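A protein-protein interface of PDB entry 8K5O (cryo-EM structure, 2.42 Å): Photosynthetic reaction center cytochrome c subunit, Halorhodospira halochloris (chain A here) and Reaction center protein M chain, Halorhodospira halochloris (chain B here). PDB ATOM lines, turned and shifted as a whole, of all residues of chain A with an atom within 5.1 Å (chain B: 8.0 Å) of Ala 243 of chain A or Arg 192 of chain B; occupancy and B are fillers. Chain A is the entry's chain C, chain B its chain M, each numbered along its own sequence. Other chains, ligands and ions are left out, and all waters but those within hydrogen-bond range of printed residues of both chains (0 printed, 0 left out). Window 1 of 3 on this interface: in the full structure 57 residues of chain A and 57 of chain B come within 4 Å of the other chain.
Among the printed residues, merely in contact across the chains: Ile 222 of chain A with Arg 192 of chain B, Val 223 of chain A with Glu 191 of chain B, Val 223 of chain A with Arg 192 of chain B, Val 223 of chain A with Gly 194 of chain B, Gly 224 of chain A with Glu 292 of chain B, Gly 237 of chain A with Arg 192 of chain B, Gly 237 of chain A with Glu 292 of chain B, Ser 239 of chain A with Asp 172 of chain B, Leu 240 of chain A with Glu 173 of chain B, Leu 240 of chain A with Trp 185 of chain B, Leu 240 of chain A with Ala 188 of chain B, Leu 240 of chain A with Ile 189 of chain B, Ala 243 of chain A with Arg 192 of chain B, Tyr 244 of chain A with Asp 184 of chain B, Tyr 244 of chain A with Trp 185 of chain B, Tyr 244 of chain A with Ala 188 of chain B and Val 247 of chain A with Val 187 of chain B.
Of the 23 printed residues of chain B, 12 touch a printed residue of chain A.
Printed residues of chain A that touch a printed residue of chain B: Ile 222, Val 223, Gly 224, Gly 237, Val 238, Ser 239, Leu 240, Arg 241, Ala 243, Tyr 244 and Val 247.
Among the printed residues, no Asp or Glu carboxylate lies within 4 Å of a Lys or Arg side-chain nitrogen of the other chain.
Of the printed residues of chain B, Gly 237 of chain A touches Arg 192 and Glu 292.
Printed residues of chain B within 4 Å of Ala 243 of chain A: Arg 192 (3.7 Å).
Of the printed residues of chain A, Trp 185 of chain B touches Leu 240 and Tyr 244.
Leu 186 of chain B touches none of the printed residues of chain A.
Printed residues of chain A within 4 Å of Ala 188 of chain B: Leu 240 (3.5 Å) and Tyr 244 (3.7 Å).
Arg 192 of chain B touches just these residues of chain A: Ile 222, Val 223, Gly 224, Gly 237, Val 238 and Ala 243.
Printed residues of chain A within 4 Å of Gly 194 of chain B: Val 223.
The nearest residue of chain B that does not touch Ala 243 of chain A is Ala 188 of chain B (4.1 Å).
The nearest residue of chain A that does not touch Arg 192 of chain B is Leu 240 of chain A (4.1 Å).
NH2 of Arg 164 of chain B is in salt-bridge range of OE1 of Glu 173 of chain B (2.7 Å).
The guanidinium group of Arg 192 of chain B is in salt-bridge range of the side-chain carboxylate of Glu 292 of chain B (3.2 Å).
The side-chain hydroxyl (OH) of Tyr 193 of chain B sits at hydrogen-bond distance from the side-chain carboxylate (OE2) of Glu 173 of chain B (2.4 Å).
The indole nitrogen of Trp 185 of chain B lies within hydrogen-bond range of the backbone carbonyl oxygen of Glu 173 of chain B (2.6 Å).
The side-chain carboxylate (OE1) of Glu 242 of chain A sits at hydrogen-bond distance from the backbone NH (N) of Ser 239 of chain A, 3.2 Å away.
The backbone carbonyl oxygen of Gly 224 of chain A sits close to the side-chain hydroxyl of Ser 293 of chain B (3.2 Å).
The backbone NH of Gly 224 of chain A lies within hydrogen-bond range of the backbone carbonyl oxygen of Arg 192 of chain B.
The backbone carbonyl oxygen (O) of Val 238 of chain A sits at hydrogen-bond distance from the guanidinium group (NE) of Arg 192 of chain B (2.6 Å).
The side-chain carboxylate (OD2) of Asp 172 of chain B lies within hydrogen-bond range of the backbone NH (N) of Leu 240 of chain A (3.5 Å).
The side-chain carboxylate (OD2) of Asp 172 of chain B sits at hydrogen-bond distance from the backbone NH (N) of Arg 241 of chain A, at 3.3 Å.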
ATOM      1  N   ILE A 222      16.484 -27.896   1.511  1.00  0.00           N
ATOM      2  CA  ILE A 222      17.550 -26.960   1.171  1.00  0.00           C
ATOM      3  C   ILE A 222      18.139 -27.184  -0.209  1.00  0.00           C
ATOM      4  O   ILE A 222      18.749 -26.257  -0.765  1.00  0.00           O
ATOM      5  CB  ILE A 222      18.702 -27.040   2.187  1.00  0.00           C
ATOM      6  CG1 ILE A 222      19.172 -28.494   2.311  1.00  0.00           C
ATOM      7  CG2 ILE A 222      18.269 -26.439   3.502  1.00  0.00           C
ATOM      8  CD1 ILE A 222      20.485 -28.674   3.007  1.00  0.00           C
ATOM      9  N   VAL A 223      17.996 -28.379  -0.776  1.00  0.00           N
ATOM     10  CA  VAL A 223      18.599 -28.656  -2.071  1.00  0.00           C
ATOM     11  C   VAL A 223      17.966 -27.757  -3.117  1.00  0.00           C
ATOM     12  O   VAL A 223      16.738 -27.612  -3.173  1.00  0.00           O
ATOM     13  CB  VAL A 223      18.445 -30.136  -2.440  1.00  0.00           C
ATOM     14  CG1 VAL A 223      19.136 -30.419  -3.757  1.00  0.00           C
ATOM     15  CG2 VAL A 223      19.011 -31.000  -1.346  1.00  0.00           C
ATOM     16  N   GLY A 224      18.804 -27.130  -3.933  1.00  0.00           N
ATOM     17  CA  GLY A 224      18.287 -26.279  -4.981  1.00  0.00           C
ATOM     18  C   GLY A 224      17.424 -27.062  -5.949  1.00  0.00           C
ATOM     19  O   GLY A 224      17.583 -28.269  -6.124  1.00  0.00           O
ATOM     20  N   GLY A 237      16.149 -19.837  -3.525  1.00  0.00           N
ATOM     21  CA  GLY A 237      16.496 -20.942  -2.670  1.00  0.00           C
ATOM     22  C   GLY A 237      16.771 -20.497  -1.249  1.00  0.00           C
ATOM     23  O   GLY A 237      16.482 -19.369  -0.847  1.00  0.00           O
ATOM     24  N   VAL A 238      17.344 -21.410  -0.485  1.00  0.00           N
ATOM     25  CA  VAL A 238      17.760 -21.118   0.867  1.00  0.00           C
ATOM     26  C   VAL A 238      19.202 -20.637   0.828  1.00  0.00           C
ATOM     27  O   VAL A 238      19.932 -20.840  -0.145  1.00  0.00           O
ATOM     28  CB  VAL A 238      17.604 -22.335   1.801  1.00  0.00           C
ATOM     29  CG1 VAL A 238      16.165 -22.803   1.818  1.00  0.00           C
ATOM     30  CG2 VAL A 238      18.531 -23.448   1.367  1.00  0.00           C
ATOM     31  N   SER A 239      19.611 -19.968   1.895  1.00  0.00           N
ATOM     32  CA  SER A 239      20.997 -19.570   2.028  1.00  0.00           C
ATOM     33  C   SER A 239      21.861 -20.789   2.335  1.00  0.00           C
ATOM     34  O   SER A 239      21.368 -21.863   2.686  1.00  0.00           O
ATOM     35  CB  SER A 239      21.143 -18.521   3.122  1.00  0.00           C
ATOM     36  OG  SER A 239      20.818 -19.056   4.391  1.00  0.00           O
ATOM     37  N   LEU A 240      23.174 -20.620   2.182  1.00  0.00           N
ATOM     38  CA  LEU A 240      24.080 -21.699   2.546  1.00  0.00           C
ATOM     39  C   LEU A 240      24.009 -21.998   4.035  1.00  0.00           C
ATOM     40  O   LEU A 240      24.196 -23.147   4.441  1.00  0.00           O
ATOM     41  CB  LEU A 240      25.513 -21.362   2.145  1.00  0.00           C
ATOM     42  CG  LEU A 240      26.435 -22.578   2.225  1.00  0.00           C
ATOM     43  CD1 LEU A 240      26.045 -23.589   1.163  1.00  0.00           C
ATOM     44  CD2 LEU A 240      27.887 -22.185   2.104  1.00  0.00           C
ATOM     45  N   ARG A 241      23.742 -20.986   4.860  1.00  0.00           N
ATOM     46  CA  ARG A 241      23.585 -21.220   6.291  1.00  0.00           C
ATOM     47  C   ARG A 241      22.365 -22.083   6.581  1.00  0.00           C
ATOM     48  O   ARG A 241      22.397 -22.932   7.477  1.00  0.00           O
ATOM     49  CB  ARG A 241      23.486 -19.893   7.031  1.00  0.00           C
ATOM     50  CG  ARG A 241      23.392 -20.035   8.530  1.00  0.00           C
ATOM     51  CD  ARG A 241      24.697 -20.532   9.103  1.00  0.00           C
ATOM     52  NE  ARG A 241      25.812 -19.672   8.733  1.00  0.00           N
ATOM     53  CZ  ARG A 241      26.314 -18.720   9.508  1.00  0.00           C
ATOM     54  NH1 ARG A 241      25.827 -18.482  10.712  1.00  0.00           N
ATOM     55  NH2 ARG A 241      27.331 -17.992   9.063  1.00  0.00           N
ATOM     56  N   GLU A 242      21.270 -21.862   5.853  1.00  0.00           N
ATOM     57  CA  GLU A 242      20.106 -22.723   6.010  1.00  0.00           C
ATOM     58  C   GLU A 242      20.438 -24.152   5.608  1.00  0.00           C
ATOM     59  O   GLU A 242      19.962 -25.109   6.229  1.00  0.00           O
ATOM     60  CB  GLU A 242      18.937 -22.176   5.195  1.00  0.00           C
ATOM     61  CG  GLU A 242      18.076 -21.192   5.966  1.00  0.00           C
ATOM     62  CD  GLU A 242      17.134 -20.407   5.080  1.00  0.00           C
ATOM     63  OE1 GLU A 242      17.614 -19.545   4.314  1.00  0.00           O
ATOM     64  OE2 GLU A 242      15.911 -20.644   5.156  1.00  0.00           O
ATOM     65  N   ALA A 243      21.270 -24.312   4.577  1.00  0.00           N
ATOM     66  CA  ALA A 243      21.760 -25.637   4.213  1.00  0.00           C
ATOM     67  C   ALA A 243      22.587 -26.245   5.337  1.00  0.00           C
ATOM     68  O   ALA A 243      22.465 -27.438   5.627  1.00  0.00           O
ATOM     69  CB  ALA A 243      22.575 -25.559   2.924  1.00  0.00           C
ATOM     70  N   TYR A 244      23.439 -25.439   5.970  1.00  0.00           N
ATOM     71  CA  TYR A 244      24.204 -25.897   7.126  1.00  0.00           C
ATOM     72  C   TYR A 244      23.283 -26.405   8.222  1.00  0.00           C
ATOM     73  O   TYR A 244      23.493 -27.489   8.772  1.00  0.00           O
ATOM     74  CB  TYR A 244      25.056 -24.757   7.676  1.00  0.00           C
ATOM     75  CG  TYR A 244      26.367 -24.506   6.985  1.00  0.00           C
ATOM     76  CD1 TYR A 244      27.409 -25.415   7.064  1.00  0.00           C
ATOM     77  CD2 TYR A 244      26.572 -23.336   6.278  1.00  0.00           C
ATOM     78  CE1 TYR A 244      28.613 -25.164   6.441  1.00  0.00           C
ATOM     79  CE2 TYR A 244      27.757 -23.081   5.654  1.00  0.00           C
ATOM     80  CZ  TYR A 244      28.775 -23.994   5.736  1.00  0.00           C
ATOM     81  OH  TYR A 244      29.956 -23.709   5.109  1.00  0.00           O
ATOM     82  N   GLU A 245      22.267 -25.614   8.567  1.00  0.00           N
ATOM     83  CA  GLU A 245      21.356 -25.987   9.644  1.00  0.00           C
ATOM     84  C   GLU A 245      20.592 -27.258   9.308  1.00  0.00           C
ATOM     85  O   GLU A 245      20.423 -28.136  10.162  1.00  0.00           O
ATOM     86  CB  GLU A 245      20.381 -24.846   9.931  1.00  0.00           C
ATOM     87  CG  GLU A 245      21.034 -23.539  10.326  1.00  0.00           C
ATOM     88  CD  GLU A 245      20.212 -22.336   9.904  1.00  0.00           C
ATOM     89  OE1 GLU A 245      19.070 -22.529   9.437  1.00  0.00           O
ATOM     90  OE2 GLU A 245      20.704 -21.196  10.039  1.00  0.00           O
ATOM     91  N   ALA A 246      20.114 -27.373   8.067  1.00  0.00           N
ATOM     92  CA  ALA A 246      19.366 -28.562   7.681  1.00  0.00           C
ATOM     93  C   ALA A 246      20.254 -29.796   7.675  1.00  0.00           C
ATOM     94  O   ALA A 246      19.834 -30.870   8.114  1.00  0.00           O
ATOM     95  CB  ALA A 246      18.720 -28.359   6.316  1.00  0.00           C
ATOM     96  N   VAL A 247      21.488 -29.664   7.184  1.00  0.00           N
ATOM     97  CA  VAL A 247      22.408 -30.793   7.196  1.00  0.00           C
ATOM     98  C   VAL A 247      22.793 -31.154   8.621  1.00  0.00           C
ATOM     99  O   VAL A 247      23.011 -32.326   8.928  1.00  0.00           O
ATOM    100  CB  VAL A 247      23.639 -30.495   6.321  1.00  0.00           C
ATOM    101  CG1 VAL A 247      24.691 -31.569   6.495  1.00  0.00           C
ATOM    102  CG2 VAL A 247      23.234 -30.410   4.865  1.00  0.00           C
ATOM    103  N   GLY A 248      22.871 -30.174   9.520  1.00  0.00           N
ATOM    104  CA  GLY A 248      23.092 -30.490  10.920  1.00  0.00           C
ATOM    105  C   GLY A 248      21.937 -31.259  11.531  1.00  0.00           C
ATOM    106  O   GLY A 248      22.141 -32.220  12.279  1.00  0.00           O
ATOM    107  N   ARG B 164      32.890 -15.594  -5.619  1.00  0.00           N
ATOM    108  CA  ARG B 164      31.614 -16.280  -5.743  1.00  0.00           C
ATOM    109  C   ARG B 164      30.651 -15.904  -4.620  1.00  0.00           C
ATOM    110  O   ARG B 164      29.449 -15.783  -4.875  1.00  0.00           O
ATOM    111  CB  ARG B 164      31.830 -17.790  -5.794  1.00  0.00           C
ATOM    112  CG  ARG B 164      30.580 -18.588  -5.976  1.00  0.00           C
ATOM    113  CD  ARG B 164      30.785 -19.966  -5.454  1.00  0.00           C
ATOM    114  NE  ARG B 164      29.522 -20.634  -5.190  1.00  0.00           N
ATOM    115  CZ  ARG B 164      29.076 -20.928  -3.980  1.00  0.00           C
ATOM    116  NH1 ARG B 164      29.772 -20.630  -2.896  1.00  0.00           N
ATOM    117  NH2 ARG B 164      27.899 -21.524  -3.854  1.00  0.00           N
ATOM    118  N   ILE B 168      27.084 -14.339  -5.654  1.00  0.00           N
ATOM    119  CA  ILE B 168      25.848 -14.797  -5.031  1.00  0.00           C
ATOM    120  C   ILE B 168      25.240 -13.698  -4.170  1.00  0.00           C
ATOM    121  O   ILE B 168      24.017 -13.640  -3.995  1.00  0.00           O
ATOM    122  CB  ILE B 168      26.110 -16.089  -4.234  1.00  0.00           C
ATOM    123  CG1 ILE B 168      26.491 -17.212  -5.193  1.00  0.00           C
ATOM    124  CG2 ILE B 168      24.907 -16.489  -3.401  1.00  0.00           C
ATOM    125  CD1 ILE B 168      26.937 -18.444  -4.510  1.00  0.00           C
ATOM    126  N   ASP B 172      27.878 -15.791   3.612  1.00  0.00           N
ATOM    127  CA  ASP B 172      27.768 -17.130   4.177  1.00  0.00           C
ATOM    128  C   ASP B 172      28.121 -18.216   3.172  1.00  0.00           C
ATOM    129  O   ASP B 172      28.332 -19.363   3.574  1.00  0.00           O
ATOM    130  CB  ASP B 172      26.364 -17.387   4.733  1.00  0.00           C
ATOM    131  CG  ASP B 172      25.296 -17.405   3.661  1.00  0.00           C
ATOM    132  OD1 ASP B 172      25.581 -17.052   2.501  1.00  0.00           O
ATOM    133  OD2 ASP B 172      24.166 -17.815   3.977  1.00  0.00           O
ATOM    134  N   GLU B 173      28.175 -17.881   1.885  1.00  0.00           N
ATOM    135  CA  GLU B 173      28.641 -18.804   0.864  1.00  0.00           C
ATOM    136  C   GLU B 173      30.145 -19.007   0.907  1.00  0.00           C
ATOM    137  O   GLU B 173      30.648 -19.928   0.258  1.00  0.00           O
ATOM    138  CB  GLU B 173      28.233 -18.302  -0.520  1.00  0.00           C
ATOM    139  CG  GLU B 173      26.737 -18.258  -0.733  1.00  0.00           C
ATOM    140  CD  GLU B 173      26.157 -19.612  -1.079  1.00  0.00           C
ATOM    141  OE1 GLU B 173      26.916 -20.482  -1.544  1.00  0.00           O
ATOM    142  OE2 GLU B 173      24.940 -19.805  -0.898  1.00  0.00           O
ATOM    143  N   ASP B 184      32.660 -29.028   6.058  1.00  0.00           N
ATOM    144  CA  ASP B 184      31.251 -28.864   6.195  1.00  0.00           C
ATOM    145  C   ASP B 184      30.797 -27.899   5.143  1.00  0.00           C
ATOM    146  O   ASP B 184      29.707 -28.001   4.719  1.00  0.00           O
ATOM    147  CB  ASP B 184      30.951 -28.389   7.615  1.00  0.00           C
ATOM    148  CG  ASP B 184      31.109 -29.426   8.600  1.00  0.00           C
ATOM    149  OD1 ASP B 184      31.806 -30.379   8.300  1.00  0.00           O
ATOM    150  OD2 ASP B 184      30.549 -29.307   9.678  1.00  0.00           O
ATOM    151  N   TRP B 185      31.608 -26.924   4.771  1.00  0.00           N
ATOM    152  CA  TRP B 185      31.307 -26.046   3.648  1.00  0.00           C
ATOM    153  C   TRP B 185      31.218 -26.834   2.357  1.00  0.00           C
ATOM    154  O   TRP B 185      30.344 -26.579   1.526  1.00  0.00           O
ATOM    155  CB  TRP B 185      32.368 -24.960   3.529  1.00  0.00           C
ATOM    156  CG  TRP B 185      32.168 -24.015   2.386  1.00  0.00           C
ATOM    157  CD1 TRP B 185      31.484 -22.844   2.410  1.00  0.00           C
ATOM    158  CD2 TRP B 185      32.685 -24.149   1.057  1.00  0.00           C
ATOM    159  NE1 TRP B 185      31.532 -22.239   1.183  1.00  0.00           N
ATOM    160  CE2 TRP B 185      32.268 -23.021   0.333  1.00  0.00           C
ATOM    161  CE3 TRP B 185      33.457 -25.118   0.408  1.00  0.00           C
ATOM    162  CZ2 TRP B 185      32.589 -22.835  -1.007  1.00  0.00           C
ATOM    163  CZ3 TRP B 185      33.782 -24.926  -0.915  1.00  0.00           C
ATOM    164  CH2 TRP B 185      33.346 -23.798  -1.610  1.00  0.00           C
ATOM    165  N   LEU B 186      32.138 -27.774   2.157  1.00  0.00           N
ATOM    166  CA  LEU B 186      32.046 -28.670   1.010  1.00  0.00           C
ATOM    167  C   LEU B 186      30.693 -29.367   0.965  1.00  0.00           C
ATOM    168  O   LEU B 186      30.005 -29.354  -0.064  1.00  0.00           O
ATOM    169  CB  LEU B 186      33.170 -29.698   1.067  1.00  0.00           C
ATOM    170  CG  LEU B 186      34.552 -29.081   0.973  1.00  0.00           C
ATOM    171  CD1 LEU B 186      35.619 -30.127   1.137  1.00  0.00           C
ATOM    172  CD2 LEU B 186      34.633 -28.427  -0.364  1.00  0.00           C
ATOM    173  N   VAL B 187      30.299 -29.980   2.082  1.00  0.00           N
ATOM    174  CA  VAL B 187      29.022 -30.693   2.123  1.00  0.00           C
ATOM    175  C   VAL B 187      27.866 -29.744   1.849  1.00  0.00           C
ATOM    176  O   VAL B 187      26.970 -30.046   1.053  1.00  0.00           O
ATOM    177  CB  VAL B 187      28.844 -31.416   3.470  1.00  0.00           C
ATOM    178  CG1 VAL B 187      27.400 -31.839   3.652  1.00  0.00           C
ATOM    179  CG2 VAL B 187      29.723 -32.626   3.521  1.00  0.00           C
ATOM    180  N   ALA B 188      27.870 -28.582   2.498  1.00  0.00           N
ATOM    181  CA  ALA B 188      26.761 -27.648   2.375  1.00  0.00           C
ATOM    182  C   ALA B 188      26.640 -27.112   0.957  1.00  0.00           C
ATOM    183  O   ALA B 188      25.532 -26.986   0.432  1.00  0.00           O
ATOM    184  CB  ALA B 188      26.930 -26.506   3.375  1.00  0.00           C
ATOM    185  N   ILE B 189      27.765 -26.782   0.322  1.00  0.00           N
ATOM    186  CA  ILE B 189      27.724 -26.293  -1.048  1.00  0.00           C
ATOM    187  C   ILE B 189      27.231 -27.380  -1.986  1.00  0.00           C
ATOM    188  O   ILE B 189      26.365 -27.138  -2.835  1.00  0.00           O
ATOM    189  CB  ILE B 189      29.103 -25.768  -1.480  1.00  0.00           C
ATOM    190  CG1 ILE B 189      29.461 -24.501  -0.715  1.00  0.00           C
ATOM    191  CG2 ILE B 189      29.107 -25.480  -2.966  1.00  0.00           C
ATOM    192  CD1 ILE B 189      28.714 -23.290  -1.186  1.00  0.00           C
ATOM    193  N   SER B 190      27.763 -28.593  -1.854  1.00  0.00           N
ATOM    194  CA  SER B 190      27.382 -29.646  -2.785  1.00  0.00           C
ATOM    195  C   SER B 190      25.912 -30.009  -2.642  1.00  0.00           C
ATOM    196  O   SER B 190      25.232 -30.248  -3.643  1.00  0.00           O
ATOM    197  CB  SER B 190      28.262 -30.871  -2.581  1.00  0.00           C
ATOM    198  OG  SER B 190      27.907 -31.917  -3.461  1.00  0.00           O
ATOM    199  N   GLU B 191      25.398 -30.054  -1.412  1.00  0.00           N
ATOM    200  CA  GLU B 191      24.023 -30.499  -1.235  1.00  0.00           C
ATOM    201  C   GLU B 191      23.024 -29.370  -1.440  1.00  0.00           C
ATOM    202  O   GLU B 191      21.916 -29.606  -1.934  1.00  0.00           O
ATOM    203  CB  GLU B 191      23.850 -31.140   0.141  1.00  0.00           C
ATOM    204  CG  GLU B 191      24.912 -32.184   0.465  1.00  0.00           C
ATOM    205  CD  GLU B 191      25.200 -33.153  -0.676  1.00  0.00           C
ATOM    206  OE1 GLU B 191      24.295 -33.469  -1.474  1.00  0.00           O
ATOM    207  OE2 GLU B 191      26.349 -33.611  -0.777  1.00  0.00           O
ATOM    208  N   ARG B 192      23.388 -28.143  -1.071  1.00  0.00           N
ATOM    209  CA  ARG B 192      22.527 -27.004  -1.352  1.00  0.00           C
ATOM    210  C   ARG B 192      22.344 -26.821  -2.852  1.00  0.00           C
ATOM    211  O   ARG B 192      21.229 -26.584  -3.328  1.00  0.00           O
ATOM    212  CB  ARG B 192      23.112 -25.742  -0.722  1.00  0.00           C
ATOM    213  CG  ARG B 192      22.673 -24.458  -1.380  1.00  0.00           C
ATOM    214  CD  ARG B 192      21.277 -24.078  -0.939  1.00  0.00           C
ATOM    215  NE  ARG B 192      20.837 -22.817  -1.521  1.00  0.00           N
ATOM    216  CZ  ARG B 192      20.243 -22.701  -2.699  1.00  0.00           C
ATOM    217  NH1 ARG B 192      19.985 -23.756  -3.451  1.00  0.00           N
ATOM    218  NH2 ARG B 192      19.901 -21.494  -3.136  1.00  0.00           N
ATOM    219  N   TYR B 193      23.428 -26.930  -3.612  1.00  0.00           N
ATOM    220  CA  TYR B 193      23.378 -26.777  -5.061  1.00  0.00           C
ATOM    221  C   TYR B 193      23.397 -28.146  -5.732  1.00  0.00           C
ATOM    222  O   TYR B 193      24.343 -28.536  -6.410  1.00  0.00           O
ATOM    223  CB  TYR B 193      24.516 -25.881  -5.529  1.00  0.00           C
ATOM    224  CG  TYR B 193      24.444 -24.548  -4.847  1.00  0.00           C
ATOM    225  CD1 TYR B 193      23.399 -23.684  -5.110  1.00  0.00           C
ATOM    226  CD2 TYR B 193      25.381 -24.174  -3.900  1.00  0.00           C
ATOM    227  CE1 TYR B 193      23.300 -22.477  -4.480  1.00  0.00           C
ATOM    228  CE2 TYR B 193      25.290 -22.963  -3.264  1.00  0.00           C
ATOM    229  CZ  TYR B 193      24.248 -22.115  -3.562  1.00  0.00           C
ATOM    230  OH  TYR B 193      24.147 -20.900  -2.933  1.00  0.00           O
ATOM    231  N   GLY B 194      22.305 -28.874  -5.527  1.00  0.00           N
ATOM    232  CA  GLY B 194      22.159 -30.171  -6.147  1.00  0.00           C
ATOM    233  C   GLY B 194      23.148 -31.176  -5.609  1.00  0.00           C
ATOM    234  O   GLY B 194      23.003 -31.673  -4.489  1.00  0.00           O
ATOM    235  N   ASN B 195      24.154 -31.491  -6.415  1.00  0.00           N
ATOM    236  CA  ASN B 195      25.175 -32.467  -6.049  1.00  0.00           C
ATOM    237  C   ASN B 195      26.387 -32.215  -6.927  1.00  0.00           C
ATOM    238  O   ASN B 195      26.276 -32.303  -8.153  1.00  0.00           O
ATOM    239  CB  ASN B 195      24.639 -33.880  -6.255  1.00  0.00           C
ATOM    240  CG  ASN B 195      25.604 -34.943  -5.815  1.00  0.00           C
ATOM    241  OD1 ASN B 195      26.646 -34.657  -5.233  1.00  0.00           O
ATOM    242  ND2 ASN B 195      25.276 -36.186  -6.117  1.00  0.00           N
ATOM    243  N   PHE B 196      27.544 -31.918  -6.325  1.00  0.00           N
ATOM    244  CA  PHE B 196      28.703 -31.679  -7.177  1.00  0.00           C
ATOM    245  C   PHE B 196      29.173 -32.924  -7.904  1.00  0.00           C
ATOM    246  O   PHE B 196      29.918 -32.802  -8.876  1.00  0.00           O
ATOM    247  CB  PHE B 196      29.897 -31.085  -6.431  1.00  0.00           C
ATOM    248  CG  PHE B 196      29.803 -29.617  -6.232  1.00  0.00           C
ATOM    249  CD1 PHE B 196      28.625 -28.949  -6.487  1.00  0.00           C
ATOM    250  CD2 PHE B 196      30.941 -28.877  -6.004  1.00  0.00           C
ATOM    251  CE1 PHE B 196      28.551 -27.599  -6.348  1.00  0.00           C
ATOM    252  CE2 PHE B 196      30.879 -27.514  -5.898  1.00  0.00           C
ATOM    253  CZ  PHE B 196      29.685 -26.876  -6.068  1.00  0.00           C
ATOM    254  N   SER B 287      27.873 -22.871  -9.483  1.00  0.00           N
ATOM    255  CA  SER B 287      27.023 -23.362  -8.406  1.00  0.00           C
ATOM    256  C   SER B 287      26.579 -22.191  -7.538  1.00  0.00           C
ATOM    257  O   SER B 287      27.361 -21.668  -6.740  1.00  0.00           O
ATOM    258  CB  SER B 287      27.779 -24.395  -7.582  1.00  0.00           C
ATOM    259  OG  SER B 287      28.169 -25.478  -8.399  1.00  0.00           O
ATOM    260  N   GLY B 288      25.323 -21.784  -7.680  1.00  0.00           N
ATOM    261  CA  GLY B 288      24.776 -20.684  -6.928  1.00  0.00           C
ATOM    262  C   GLY B 288      24.613 -19.400  -7.708  1.00  0.00           C
ATOM    263  O   GLY B 288      23.924 -18.490  -7.235  1.00  0.00           O
ATOM    264  N   ILE B 291      23.688 -22.264 -11.702  1.00  0.00           N
ATOM    265  CA  ILE B 291      23.140 -23.580 -11.410  1.00  0.00           C
ATOM    266  C   ILE B 291      22.572 -23.563 -10.002  1.00  0.00           C
ATOM    267  O   ILE B 291      23.270 -23.209  -9.044  1.00  0.00           O
ATOM    268  CB  ILE B 291      24.213 -24.669 -11.565  1.00  0.00           C
ATOM    269  CG1 ILE B 291      24.905 -24.516 -12.917  1.00  0.00           C
ATOM    270  CG2 ILE B 291      23.612 -26.054 -11.399  1.00  0.00           C
ATOM    271  CD1 ILE B 291      24.092 -25.010 -14.074  1.00  0.00           C
ATOM    272  N   GLU B 292      21.304 -23.934  -9.876  1.00  0.00           N
ATOM    273  CA  GLU B 292      20.693 -24.079  -8.564  1.00  0.00           C
ATOM    274  C   GLU B 292      20.742 -25.513  -8.066  1.00  0.00           C
ATOM    275  O   GLU B 292      20.915 -25.741  -6.866  1.00  0.00           O
ATOM    276  CB  GLU B 292      19.246 -23.581  -8.596  1.00  0.00           C
ATOM    277  CG  GLU B 292      18.562 -23.595  -7.249  1.00  0.00           C
ATOM    278  CD  GLU B 292      18.855 -22.364  -6.421  1.00  0.00           C
ATOM    279  OE1 GLU B 292      19.958 -21.794  -6.556  1.00  0.00           O
ATOM    280  OE2 GLU B 292      17.981 -21.964  -5.625  1.00  0.00           O
ATOM    281  N   SER B 293      20.609 -26.482  -8.965  1.00  0.00           N
ATOM    282  CA  SER B 293      20.748 -27.892  -8.630  1.00  0.00           C
ATOM    283  C   SER B 293      21.543 -28.564  -9.732  1.00  0.00           C
ATOM    284  O   SER B 293      21.127 -28.544 -10.893  1.00  0.00           O
ATOM    285  CB  SER B 293      19.388 -28.568  -8.478  1.00  0.00           C
ATOM    286  OG  SER B 293      19.530 -29.908  -8.043  1.00  0.00           O
ATOM    287  N   TRP B 294      22.681 -29.150  -9.375  1.00  0.00           N
ATOM    288  CA  TRP B 294      23.413 -29.936 -10.356  1.00  0.00           C
ATOM    289  C   TRP B 294      22.697 -31.238 -10.658  1.00  0.00           C
ATOM    290  O   TRP B 294      22.826 -31.772 -11.761  1.00  0.00           O
ATOM    291  CB  TRP B 294      24.828 -30.208  -9.865  1.00  0.00           C
ATOM    292  CG  TRP B 294      25.675 -29.006  -9.892  1.00  0.00           C
ATOM    293  CD1 TRP B 294      26.092 -28.276  -8.827  1.00  0.00           C
ATOM    294  CD2 TRP B 294      26.190 -28.356 -11.053  1.00  0.00           C
ATOM    295  NE1 TRP B 294      26.852 -27.218  -9.247  1.00  0.00           N
ATOM    296  CE2 TRP B 294      26.925 -27.244 -10.614  1.00  0.00           C
ATOM    297  CE3 TRP B 294      26.106 -28.612 -12.423  1.00  0.00           C
ATOM    298  CZ2 TRP B 294      27.576 -26.389 -11.495  1.00  0.00           C
ATOM    299  CZ3 TRP B 294      26.747 -27.764 -13.291  1.00  0.00           C
ATOM    300  CH2 TRP B 294      27.479 -26.669 -12.824  1.00  0.00           C
